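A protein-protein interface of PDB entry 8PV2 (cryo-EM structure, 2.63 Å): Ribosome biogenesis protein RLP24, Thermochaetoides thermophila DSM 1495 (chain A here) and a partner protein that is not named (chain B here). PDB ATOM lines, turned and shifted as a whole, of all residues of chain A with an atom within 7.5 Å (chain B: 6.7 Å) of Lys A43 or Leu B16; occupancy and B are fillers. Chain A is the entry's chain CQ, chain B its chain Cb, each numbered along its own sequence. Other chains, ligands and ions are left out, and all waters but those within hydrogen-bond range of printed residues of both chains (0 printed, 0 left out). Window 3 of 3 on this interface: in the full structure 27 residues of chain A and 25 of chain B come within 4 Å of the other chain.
Printed residues of chain B within 4 Å of Arg A23: Arg B15 (3.4 Å), Asp B18 (3.2 Å) and Gln B21 (3.6 Å). Printed residues of chain A within 4 Å of Thr B12: Lys A41 (3.9 Å). Leu B16 touches one residue of chain A. Of the printed residues of chain A, Arg B17 touches Lys A43.
Of the 12 printed residues of chain A, 3 touch a printed residue of chain B. Of the 11 printed residues of chain B, 6 touch a printed residue of chain A. Among the printed residues, Asp or Glu carboxylates within 4 Å of a Lys or Arg side-chain nitrogen of the other chain: Arg A23 with Asp B18 (3.2 Å) and Lys A43 with Asp B18 (2.4 Å).
The side-chain amino group of Lys A43 lies within hydrogen-bond range of the backbone carbonyl oxygen of Leu B16. The guanidinium group (NH1) of Arg A23 is in salt-bridge range of the side-chain carboxylate (OD2) of Asp B18 (3.2 Å). The side-chain amino group of Lys A43 sits close to the side-chain carboxylate of Asp B18 (2.4 Å).
N of Asp B18 lies within hydrogen-bond range of OE1 of Gln B21 (3.3 Å). OD2 of Asp B18 lies within salt-bridge range of NH2 of Arg B15 (2.4 Å).
Among the printed residues, pairs that only touch across the chains: Arg A23 with Arg B15, Arg A23 with Gln B21, Lys A43 with Arg B17 and Lys A41 with Thr B12.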
ATOM      1  N   PHE A   8     -15.080  -3.064 -31.994  1.00  0.00           N
ATOM      2  CA  PHE A   8     -15.414  -4.025 -30.956  1.00  0.00           C
ATOM      3  C   PHE A   8     -16.850  -4.518 -31.083  1.00  0.00           C
ATOM      4  O   PHE A   8     -17.089  -5.722 -31.219  1.00  0.00           O
ATOM      5  CB  PHE A   8     -15.166  -3.395 -29.589  1.00  0.00           C
ATOM      6  CG  PHE A   8     -14.871  -4.382 -28.511  1.00  0.00           C
ATOM      7  CD1 PHE A   8     -15.879  -4.868 -27.707  1.00  0.00           C
ATOM      8  CD2 PHE A   8     -13.579  -4.817 -28.295  1.00  0.00           C
ATOM      9  CE1 PHE A   8     -15.604  -5.774 -26.713  1.00  0.00           C
ATOM     10  CE2 PHE A   8     -13.299  -5.723 -27.299  1.00  0.00           C
ATOM     11  CZ  PHE A   8     -14.313  -6.207 -26.515  1.00  0.00           C
ATOM     12  N   ARG A  23      -1.837   1.338 -33.300  1.00  0.00           N
ATOM     13  CA  ARG A  23      -0.869   0.341 -32.874  1.00  0.00           C
ATOM     14  C   ARG A  23       0.398   0.453 -33.717  1.00  0.00           C
ATOM     15  O   ARG A  23       0.379   0.999 -34.822  1.00  0.00           O
ATOM     16  CB  ARG A  23      -1.477  -1.055 -32.989  1.00  0.00           C
ATOM     17  CG  ARG A  23      -0.937  -2.066 -32.011  1.00  0.00           C
ATOM     18  CD  ARG A  23      -1.859  -3.256 -31.917  1.00  0.00           C
ATOM     19  NE  ARG A  23      -1.947  -3.979 -33.176  1.00  0.00           N
ATOM     20  CZ  ARG A  23      -2.755  -5.006 -33.394  1.00  0.00           C
ATOM     21  NH1 ARG A  23      -3.568  -5.456 -32.453  1.00  0.00           N
ATOM     22  NH2 ARG A  23      -2.742  -5.601 -34.582  1.00  0.00           N
ATOM     23  N   HIS A  37     -13.824   0.553 -25.721  1.00  0.00           N
ATOM     24  CA  HIS A  37     -12.398   0.825 -25.572  1.00  0.00           C
ATOM     25  C   HIS A  37     -11.816   0.151 -24.329  1.00  0.00           C
ATOM     26  O   HIS A  37     -10.729  -0.438 -24.383  1.00  0.00           O
ATOM     27  CB  HIS A  37     -12.168   2.332 -25.545  1.00  0.00           C
ATOM     28  CG  HIS A  37     -10.729   2.718 -25.440  1.00  0.00           C
ATOM     29  ND1 HIS A  37     -10.289   3.727 -24.615  1.00  0.00           N
ATOM     30  CD2 HIS A  37      -9.626   2.215 -26.039  1.00  0.00           C
ATOM     31  CE1 HIS A  37      -8.978   3.839 -24.720  1.00  0.00           C
ATOM     32  NE2 HIS A  37      -8.551   2.931 -25.577  1.00  0.00           N
ATOM     33  N   LYS A  38     -12.537   0.196 -23.209  1.00  0.00           N
ATOM     34  CA  LYS A  38     -12.050  -0.401 -21.974  1.00  0.00           C
ATOM     35  C   LYS A  38     -12.079  -1.922 -22.031  1.00  0.00           C
ATOM     36  O   LYS A  38     -11.183  -2.577 -21.495  1.00  0.00           O
ATOM     37  CB  LYS A  38     -12.868   0.115 -20.790  1.00  0.00           C
ATOM     38  CG  LYS A  38     -12.524   1.534 -20.386  1.00  0.00           C
ATOM     39  CD  LYS A  38     -13.511   2.078 -19.382  1.00  0.00           C
ATOM     40  CE  LYS A  38     -13.221   3.526 -19.048  1.00  0.00           C
ATOM     41  NZ  LYS A  38     -14.120   4.038 -17.982  1.00  0.00           N
ATOM     42  N   ASN A  39     -13.092  -2.505 -22.679  1.00  0.00           N
ATOM     43  CA  ASN A  39     -13.094  -3.955 -22.862  1.00  0.00           C
ATOM     44  C   ASN A  39     -11.941  -4.402 -23.756  1.00  0.00           C
ATOM     45  O   ASN A  39     -11.298  -5.429 -23.494  1.00  0.00           O
ATOM     46  CB  ASN A  39     -14.438  -4.398 -23.429  1.00  0.00           C
ATOM     47  CG  ASN A  39     -15.498  -4.524 -22.362  1.00  0.00           C
ATOM     48  OD1 ASN A  39     -15.367  -5.318 -21.438  1.00  0.00           O
ATOM     49  ND2 ASN A  39     -16.535  -3.710 -22.459  1.00  0.00           N
ATOM     50  N   PHE A  40     -11.643  -3.617 -24.796  1.00  0.00           N
ATOM     51  CA  PHE A  40     -10.488  -3.890 -25.642  1.00  0.00           C
ATOM     52  C   PHE A  40      -9.184  -3.805 -24.858  1.00  0.00           C
ATOM     53  O   PHE A  40      -8.290  -4.637 -25.043  1.00  0.00           O
ATOM     54  CB  PHE A  40     -10.482  -2.913 -26.817  1.00  0.00           C
ATOM     55  CG  PHE A  40      -9.378  -3.141 -27.802  1.00  0.00           C
ATOM     56  CD1 PHE A  40      -9.522  -4.068 -28.815  1.00  0.00           C
ATOM     57  CD2 PHE A  40      -8.208  -2.401 -27.739  1.00  0.00           C
ATOM     58  CE1 PHE A  40      -8.516  -4.269 -29.729  1.00  0.00           C
ATOM     59  CE2 PHE A  40      -7.202  -2.599 -28.650  1.00  0.00           C
ATOM     60  CZ  PHE A  40      -7.354  -3.538 -29.644  1.00  0.00           C
ATOM     61  N   LYS A  41      -9.053  -2.808 -23.980  1.00  0.00           N
ATOM     62  CA  LYS A  41      -7.853  -2.710 -23.156  1.00  0.00           C
ATOM     63  C   LYS A  41      -7.782  -3.809 -22.105  1.00  0.00           C
ATOM     64  O   LYS A  41      -6.685  -4.143 -21.649  1.00  0.00           O
ATOM     65  CB  LYS A  41      -7.771  -1.342 -22.479  1.00  0.00           C
ATOM     66  CG  LYS A  41      -7.570  -0.188 -23.437  1.00  0.00           C
ATOM     67  CD  LYS A  41      -7.867   1.135 -22.764  1.00  0.00           C
ATOM     68  CE  LYS A  41      -6.844   1.464 -21.704  1.00  0.00           C
ATOM     69  NZ  LYS A  41      -5.521   1.795 -22.297  1.00  0.00           N
ATOM     70  N   MET A  42      -8.920  -4.365 -21.706  1.00  0.00           N
ATOM     71  CA  MET A  42      -8.958  -5.519 -20.822  1.00  0.00           C
ATOM     72  C   MET A  42      -8.822  -6.838 -21.565  1.00  0.00           C
ATOM     73  O   MET A  42      -8.866  -7.884 -20.920  1.00  0.00           O
ATOM     74  CB  MET A  42     -10.254  -5.528 -20.005  1.00  0.00           C
ATOM     75  CG  MET A  42     -10.337  -4.440 -18.958  1.00  0.00           C
ATOM     76  SD  MET A  42     -11.573  -4.765 -17.690  1.00  0.00           S
ATOM     77  CE  MET A  42     -13.068  -4.755 -18.671  1.00  0.00           C
ATOM     78  N   LYS A  43      -8.694  -6.806 -22.896  1.00  0.00           N
ATOM     79  CA  LYS A  43      -8.407  -7.990 -23.727  1.00  0.00           C
ATOM     80  C   LYS A  43      -9.576  -8.969 -23.725  1.00  0.00           C
ATOM     81  O   LYS A  43      -9.386 -10.181 -23.799  1.00  0.00           O
ATOM     82  CB  LYS A  43      -7.116  -8.717 -23.319  1.00  0.00           C
ATOM     83  CG  LYS A  43      -5.888  -7.862 -23.085  1.00  0.00           C
ATOM     84  CD  LYS A  43      -5.168  -7.514 -24.361  1.00  0.00           C
ATOM     85  CE  LYS A  43      -3.812  -6.914 -24.040  1.00  0.00           C
ATOM     86  NZ  LYS A  43      -2.960  -6.758 -25.246  1.00  0.00           N
ATOM     87  N   ARG A  44     -10.788  -8.442 -23.629  1.00  0.00           N
ATOM     88  CA  ARG A  44     -11.978  -9.260 -23.771  1.00  0.00           C
ATOM     89  C   ARG A  44     -12.236  -9.543 -25.244  1.00  0.00           C
ATOM     90  O   ARG A  44     -11.947  -8.714 -26.109  1.00  0.00           O
ATOM     91  CB  ARG A  44     -13.178  -8.556 -23.144  1.00  0.00           C
ATOM     92  CG  ARG A  44     -12.925  -8.107 -21.717  1.00  0.00           C
ATOM     93  CD  ARG A  44     -14.135  -8.326 -20.840  1.00  0.00           C
ATOM     94  NE  ARG A  44     -14.365  -9.736 -20.560  1.00  0.00           N
ATOM     95  CZ  ARG A  44     -15.416 -10.202 -19.904  1.00  0.00           C
ATOM     96  NH1 ARG A  44     -16.362  -9.395 -19.455  1.00  0.00           N
ATOM     97  NH2 ARG A  44     -15.522 -11.509 -19.695  1.00  0.00           N
ATOM     98  N   ASN A  45     -12.761 -10.728 -25.527  1.00  0.00           N
ATOM     99  CA  ASN A  45     -13.097 -11.113 -26.889  1.00  0.00           C
ATOM    100  C   ASN A  45     -14.486 -10.593 -27.229  1.00  0.00           C
ATOM    101  O   ASN A  45     -15.440 -10.906 -26.507  1.00  0.00           O
ATOM    102  CB  ASN A  45     -13.059 -12.624 -27.038  1.00  0.00           C
ATOM    103  CG  ASN A  45     -12.947 -13.075 -28.479  1.00  0.00           C
ATOM    104  OD1 ASN A  45     -13.109 -12.293 -29.407  1.00  0.00           O
ATOM    105  ND2 ASN A  45     -12.682 -14.356 -28.669  1.00  0.00           N
ATOM    106  N   PRO A  46     -14.645  -9.790 -28.289  1.00  0.00           N
ATOM    107  CA  PRO A  46     -15.999  -9.373 -28.697  1.00  0.00           C
ATOM    108  C   PRO A  46     -16.898 -10.529 -29.091  1.00  0.00           C
ATOM    109  O   PRO A  46     -18.122 -10.438 -28.946  1.00  0.00           O
ATOM    110  CB  PRO A  46     -15.733  -8.446 -29.889  1.00  0.00           C
ATOM    111  CG  PRO A  46     -14.349  -8.007 -29.733  1.00  0.00           C
ATOM    112  CD  PRO A  46     -13.605  -9.117 -29.080  1.00  0.00           C
ATOM    113  N   LYS B  11      -3.056   0.520 -17.807  1.00  0.00           N
ATOM    114  CA  LYS B  11      -2.357   1.656 -18.392  1.00  0.00           C
ATOM    115  C   LYS B  11      -1.733   1.265 -19.724  1.00  0.00           C
ATOM    116  O   LYS B  11      -1.497   0.087 -20.001  1.00  0.00           O
ATOM    117  CB  LYS B  11      -1.272   2.171 -17.445  1.00  0.00           C
ATOM    118  CG  LYS B  11      -1.771   3.140 -16.395  1.00  0.00           C
ATOM    119  CD  LYS B  11      -0.642   3.676 -15.546  1.00  0.00           C
ATOM    120  CE  LYS B  11      -1.093   4.859 -14.704  1.00  0.00           C
ATOM    121  NZ  LYS B  11      -1.226   6.108 -15.483  1.00  0.00           N
ATOM    122  N   THR B  12      -1.483   2.270 -20.563  1.00  0.00           N
ATOM    123  CA  THR B  12      -0.849   2.018 -21.851  1.00  0.00           C
ATOM    124  C   THR B  12       0.597   1.567 -21.678  1.00  0.00           C
ATOM    125  O   THR B  12       1.094   0.752 -22.460  1.00  0.00           O
ATOM    126  CB  THR B  12      -0.925   3.272 -22.726  1.00  0.00           C
ATOM    127  OG1 THR B  12      -2.255   3.799 -22.685  1.00  0.00           O
ATOM    128  CG2 THR B  12      -0.593   2.950 -24.169  1.00  0.00           C
ATOM    129  N   ARG B  14       1.720  -0.419 -19.557  1.00  0.00           N
ATOM    130  CA  ARG B  14       1.748  -1.801 -19.100  1.00  0.00           C
ATOM    131  C   ARG B  14       1.143  -2.757 -20.119  1.00  0.00           C
ATOM    132  O   ARG B  14       0.755  -3.870 -19.756  1.00  0.00           O
ATOM    133  CB  ARG B  14       1.009  -1.931 -17.770  1.00  0.00           C
ATOM    134  CG  ARG B  14       1.612  -1.134 -16.638  1.00  0.00           C
ATOM    135  CD  ARG B  14       2.592  -1.965 -15.842  1.00  0.00           C
ATOM    136  NE  ARG B  14       2.014  -3.242 -15.449  1.00  0.00           N
ATOM    137  CZ  ARG B  14       1.266  -3.425 -14.372  1.00  0.00           C
ATOM    138  NH1 ARG B  14       0.981  -2.430 -13.552  1.00  0.00           N
ATOM    139  NH2 ARG B  14       0.789  -4.637 -14.114  1.00  0.00           N
ATOM    140  N   ARG B  15       1.053  -2.348 -21.379  1.00  0.00           N
ATOM    141  CA  ARG B  15       0.265  -3.080 -22.357  1.00  0.00           C
ATOM    142  C   ARG B  15       1.019  -4.308 -22.859  1.00  0.00           C
ATOM    143  O   ARG B  15       2.235  -4.284 -23.053  1.00  0.00           O
ATOM    144  CB  ARG B  15      -0.094  -2.156 -23.520  1.00  0.00           C
ATOM    145  CG  ARG B  15      -1.049  -2.743 -24.526  1.00  0.00           C
ATOM    146  CD  ARG B  15      -1.115  -1.897 -25.769  1.00  0.00           C
ATOM    147  NE  ARG B  15      -1.728  -2.627 -26.869  1.00  0.00           N
ATOM    148  CZ  ARG B  15      -1.074  -3.434 -27.690  1.00  0.00           C
ATOM    149  NH1 ARG B  15       0.231  -3.620 -27.581  1.00  0.00           N
ATOM    150  NH2 ARG B  15      -1.741  -4.052 -28.658  1.00  0.00           N
ATOM    151  N   LEU B  16       0.276  -5.392 -23.068  1.00  0.00           N
ATOM    152  CA  LEU B  16       0.815  -6.655 -23.540  1.00  0.00           C
ATOM    153  C   LEU B  16       0.490  -6.848 -25.016  1.00  0.00           C
ATOM    154  O   LEU B  16      -0.371  -6.169 -25.580  1.00  0.00           O
ATOM    155  CB  LEU B  16       0.254  -7.829 -22.732  1.00  0.00           C
ATOM    156  CG  LEU B  16       0.356  -7.749 -21.212  1.00  0.00           C
ATOM    157  CD1 LEU B  16      -0.316  -8.953 -20.590  1.00  0.00           C
ATOM    158  CD2 LEU B  16       1.803  -7.666 -20.782  1.00  0.00           C
ATOM    159  N   ARG B  17       1.193  -7.793 -25.636  1.00  0.00           N
ATOM    160  CA  ARG B  17       0.991  -8.091 -27.048  1.00  0.00           C
ATOM    161  C   ARG B  17      -0.357  -8.764 -27.273  1.00  0.00           C
ATOM    162  O   ARG B  17      -0.805  -9.582 -26.464  1.00  0.00           O
ATOM    163  CB  ARG B  17       2.122  -8.985 -27.553  1.00  0.00           C
ATOM    164  CG  ARG B  17       2.204  -9.133 -29.055  1.00  0.00           C
ATOM    165  CD  ARG B  17       3.599  -9.556 -29.461  1.00  0.00           C
ATOM    166  NE  ARG B  17       3.743  -9.725 -30.900  1.00  0.00           N
ATOM    167  CZ  ARG B  17       3.972  -8.737 -31.753  1.00  0.00           C
ATOM    168  NH1 ARG B  17       4.061  -7.482 -31.349  1.00  0.00           N
ATOM    169  NH2 ARG B  17       4.121  -9.017 -33.043  1.00  0.00           N
ATOM    170  N   ASP B  18      -1.002  -8.421 -28.383  1.00  0.00           N
ATOM    171  CA  ASP B  18      -2.348  -8.898 -28.661  1.00  0.00           C
ATOM    172  C   ASP B  18      -2.343 -10.242 -29.378  1.00  0.00           C
ATOM    173  O   ASP B  18      -1.341 -10.668 -29.962  1.00  0.00           O
ATOM    174  CB  ASP B  18      -3.119  -7.877 -29.492  1.00  0.00           C
ATOM    175  CG  ASP B  18      -3.508  -6.653 -28.693  1.00  0.00           C
ATOM    176  OD1 ASP B  18      -3.754  -6.791 -27.478  1.00  0.00           O
ATOM    177  OD2 ASP B  18      -3.572  -5.551 -29.275  1.00  0.00           O
ATOM    178  N   LEU B  19      -3.505 -10.898 -29.344  1.00  0.00           N
ATOM    179  CA  LEU B  19      -3.625 -12.260 -29.850  1.00  0.00           C
ATOM    180  C   LEU B  19      -3.545 -12.307 -31.369  1.00  0.00           C
ATOM    181  O   LEU B  19      -3.074 -13.296 -31.938  1.00  0.00           O
ATOM    182  CB  LEU B  19      -4.933 -12.876 -29.358  1.00  0.00           C
ATOM    183  CG  LEU B  19      -5.047 -14.397 -29.405  1.00  0.00           C
ATOM    184  CD1 LEU B  19      -4.094 -15.042 -28.417  1.00  0.00           C
ATOM    185  CD2 LEU B  19      -6.472 -14.820 -29.137  1.00  0.00           C
ATOM    186  N   GLN B  21      -1.664 -10.274 -33.191  1.00  0.00           N
ATOM    187  CA  GLN B  21      -0.227 -10.201 -33.422  1.00  0.00           C
ATOM    188  C   GLN B  21       0.448 -11.531 -33.109  1.00  0.00           C
ATOM    189  O   GLN B  21       1.411 -11.913 -33.780  1.00  0.00           O
ATOM    190  CB  GLN B  21       0.379  -9.078 -32.587  1.00  0.00           C
ATOM    191  CG  GLN B  21      -0.212  -7.721 -32.881  1.00  0.00           C
ATOM    192  CD  GLN B  21       0.366  -6.631 -32.016  1.00  0.00           C
ATOM    193  OE1 GLN B  21       0.096  -6.561 -30.820  1.00  0.00           O
ATOM    194  NE2 GLN B  21       1.169  -5.767 -32.619  1.00  0.00           N
ATOM    195  N   ARG B  77      -4.055 -19.622 -23.470  1.00  0.00           N
ATOM    196  CA  ARG B  77      -3.572 -19.027 -24.712  1.00  0.00           C
ATOM    197  C   ARG B  77      -3.744 -19.980 -25.889  1.00  0.00           C
ATOM    198  O   ARG B  77      -4.126 -19.557 -26.986  1.00  0.00           O
ATOM    199  CB  ARG B  77      -2.114 -18.604 -24.568  1.00  0.00           C
ATOM    200  CG  ARG B  77      -1.965 -17.213 -24.015  1.00  0.00           C
ATOM    201  CD  ARG B  77      -2.554 -16.198 -24.972  1.00  0.00           C
ATOM    202  NE  ARG B  77      -2.825 -14.926 -24.317  1.00  0.00           N
ATOM    203  CZ  ARG B  77      -1.944 -13.945 -24.187  1.00  0.00           C
ATOM    204  NH1 ARG B  77      -0.717 -14.052 -24.662  1.00  0.00           N
ATOM    205  NH2 ARG B  77      -2.306 -12.828 -23.566  1.00  0.00           N
ATOM    206  N   GLN B  80      -7.465 -19.970 -26.819  1.00  0.00           N
ATOM    207  CA  GLN B  80      -7.842 -18.746 -27.520  1.00  0.00           C
ATOM    208  C   GLN B  80      -7.292 -18.723 -28.940  1.00  0.00           C
ATOM    209  O   GLN B  80      -7.954 -18.228 -29.857  1.00  0.00           O
ATOM    210  CB  GLN B  80      -7.357 -17.530 -26.739  1.00  0.00           C
ATOM    211  CG  GLN B  80      -8.170 -17.235 -25.504  1.00  0.00           C
ATOM    212  CD  GLN B  80      -7.573 -16.129 -24.674  1.00  0.00           C
ATOM    213  OE1 GLN B  80      -6.485 -15.643 -24.963  1.00  0.00           O
ATOM    214  NE2 GLN B  80      -8.274 -15.737 -23.622  1.00  0.00           N
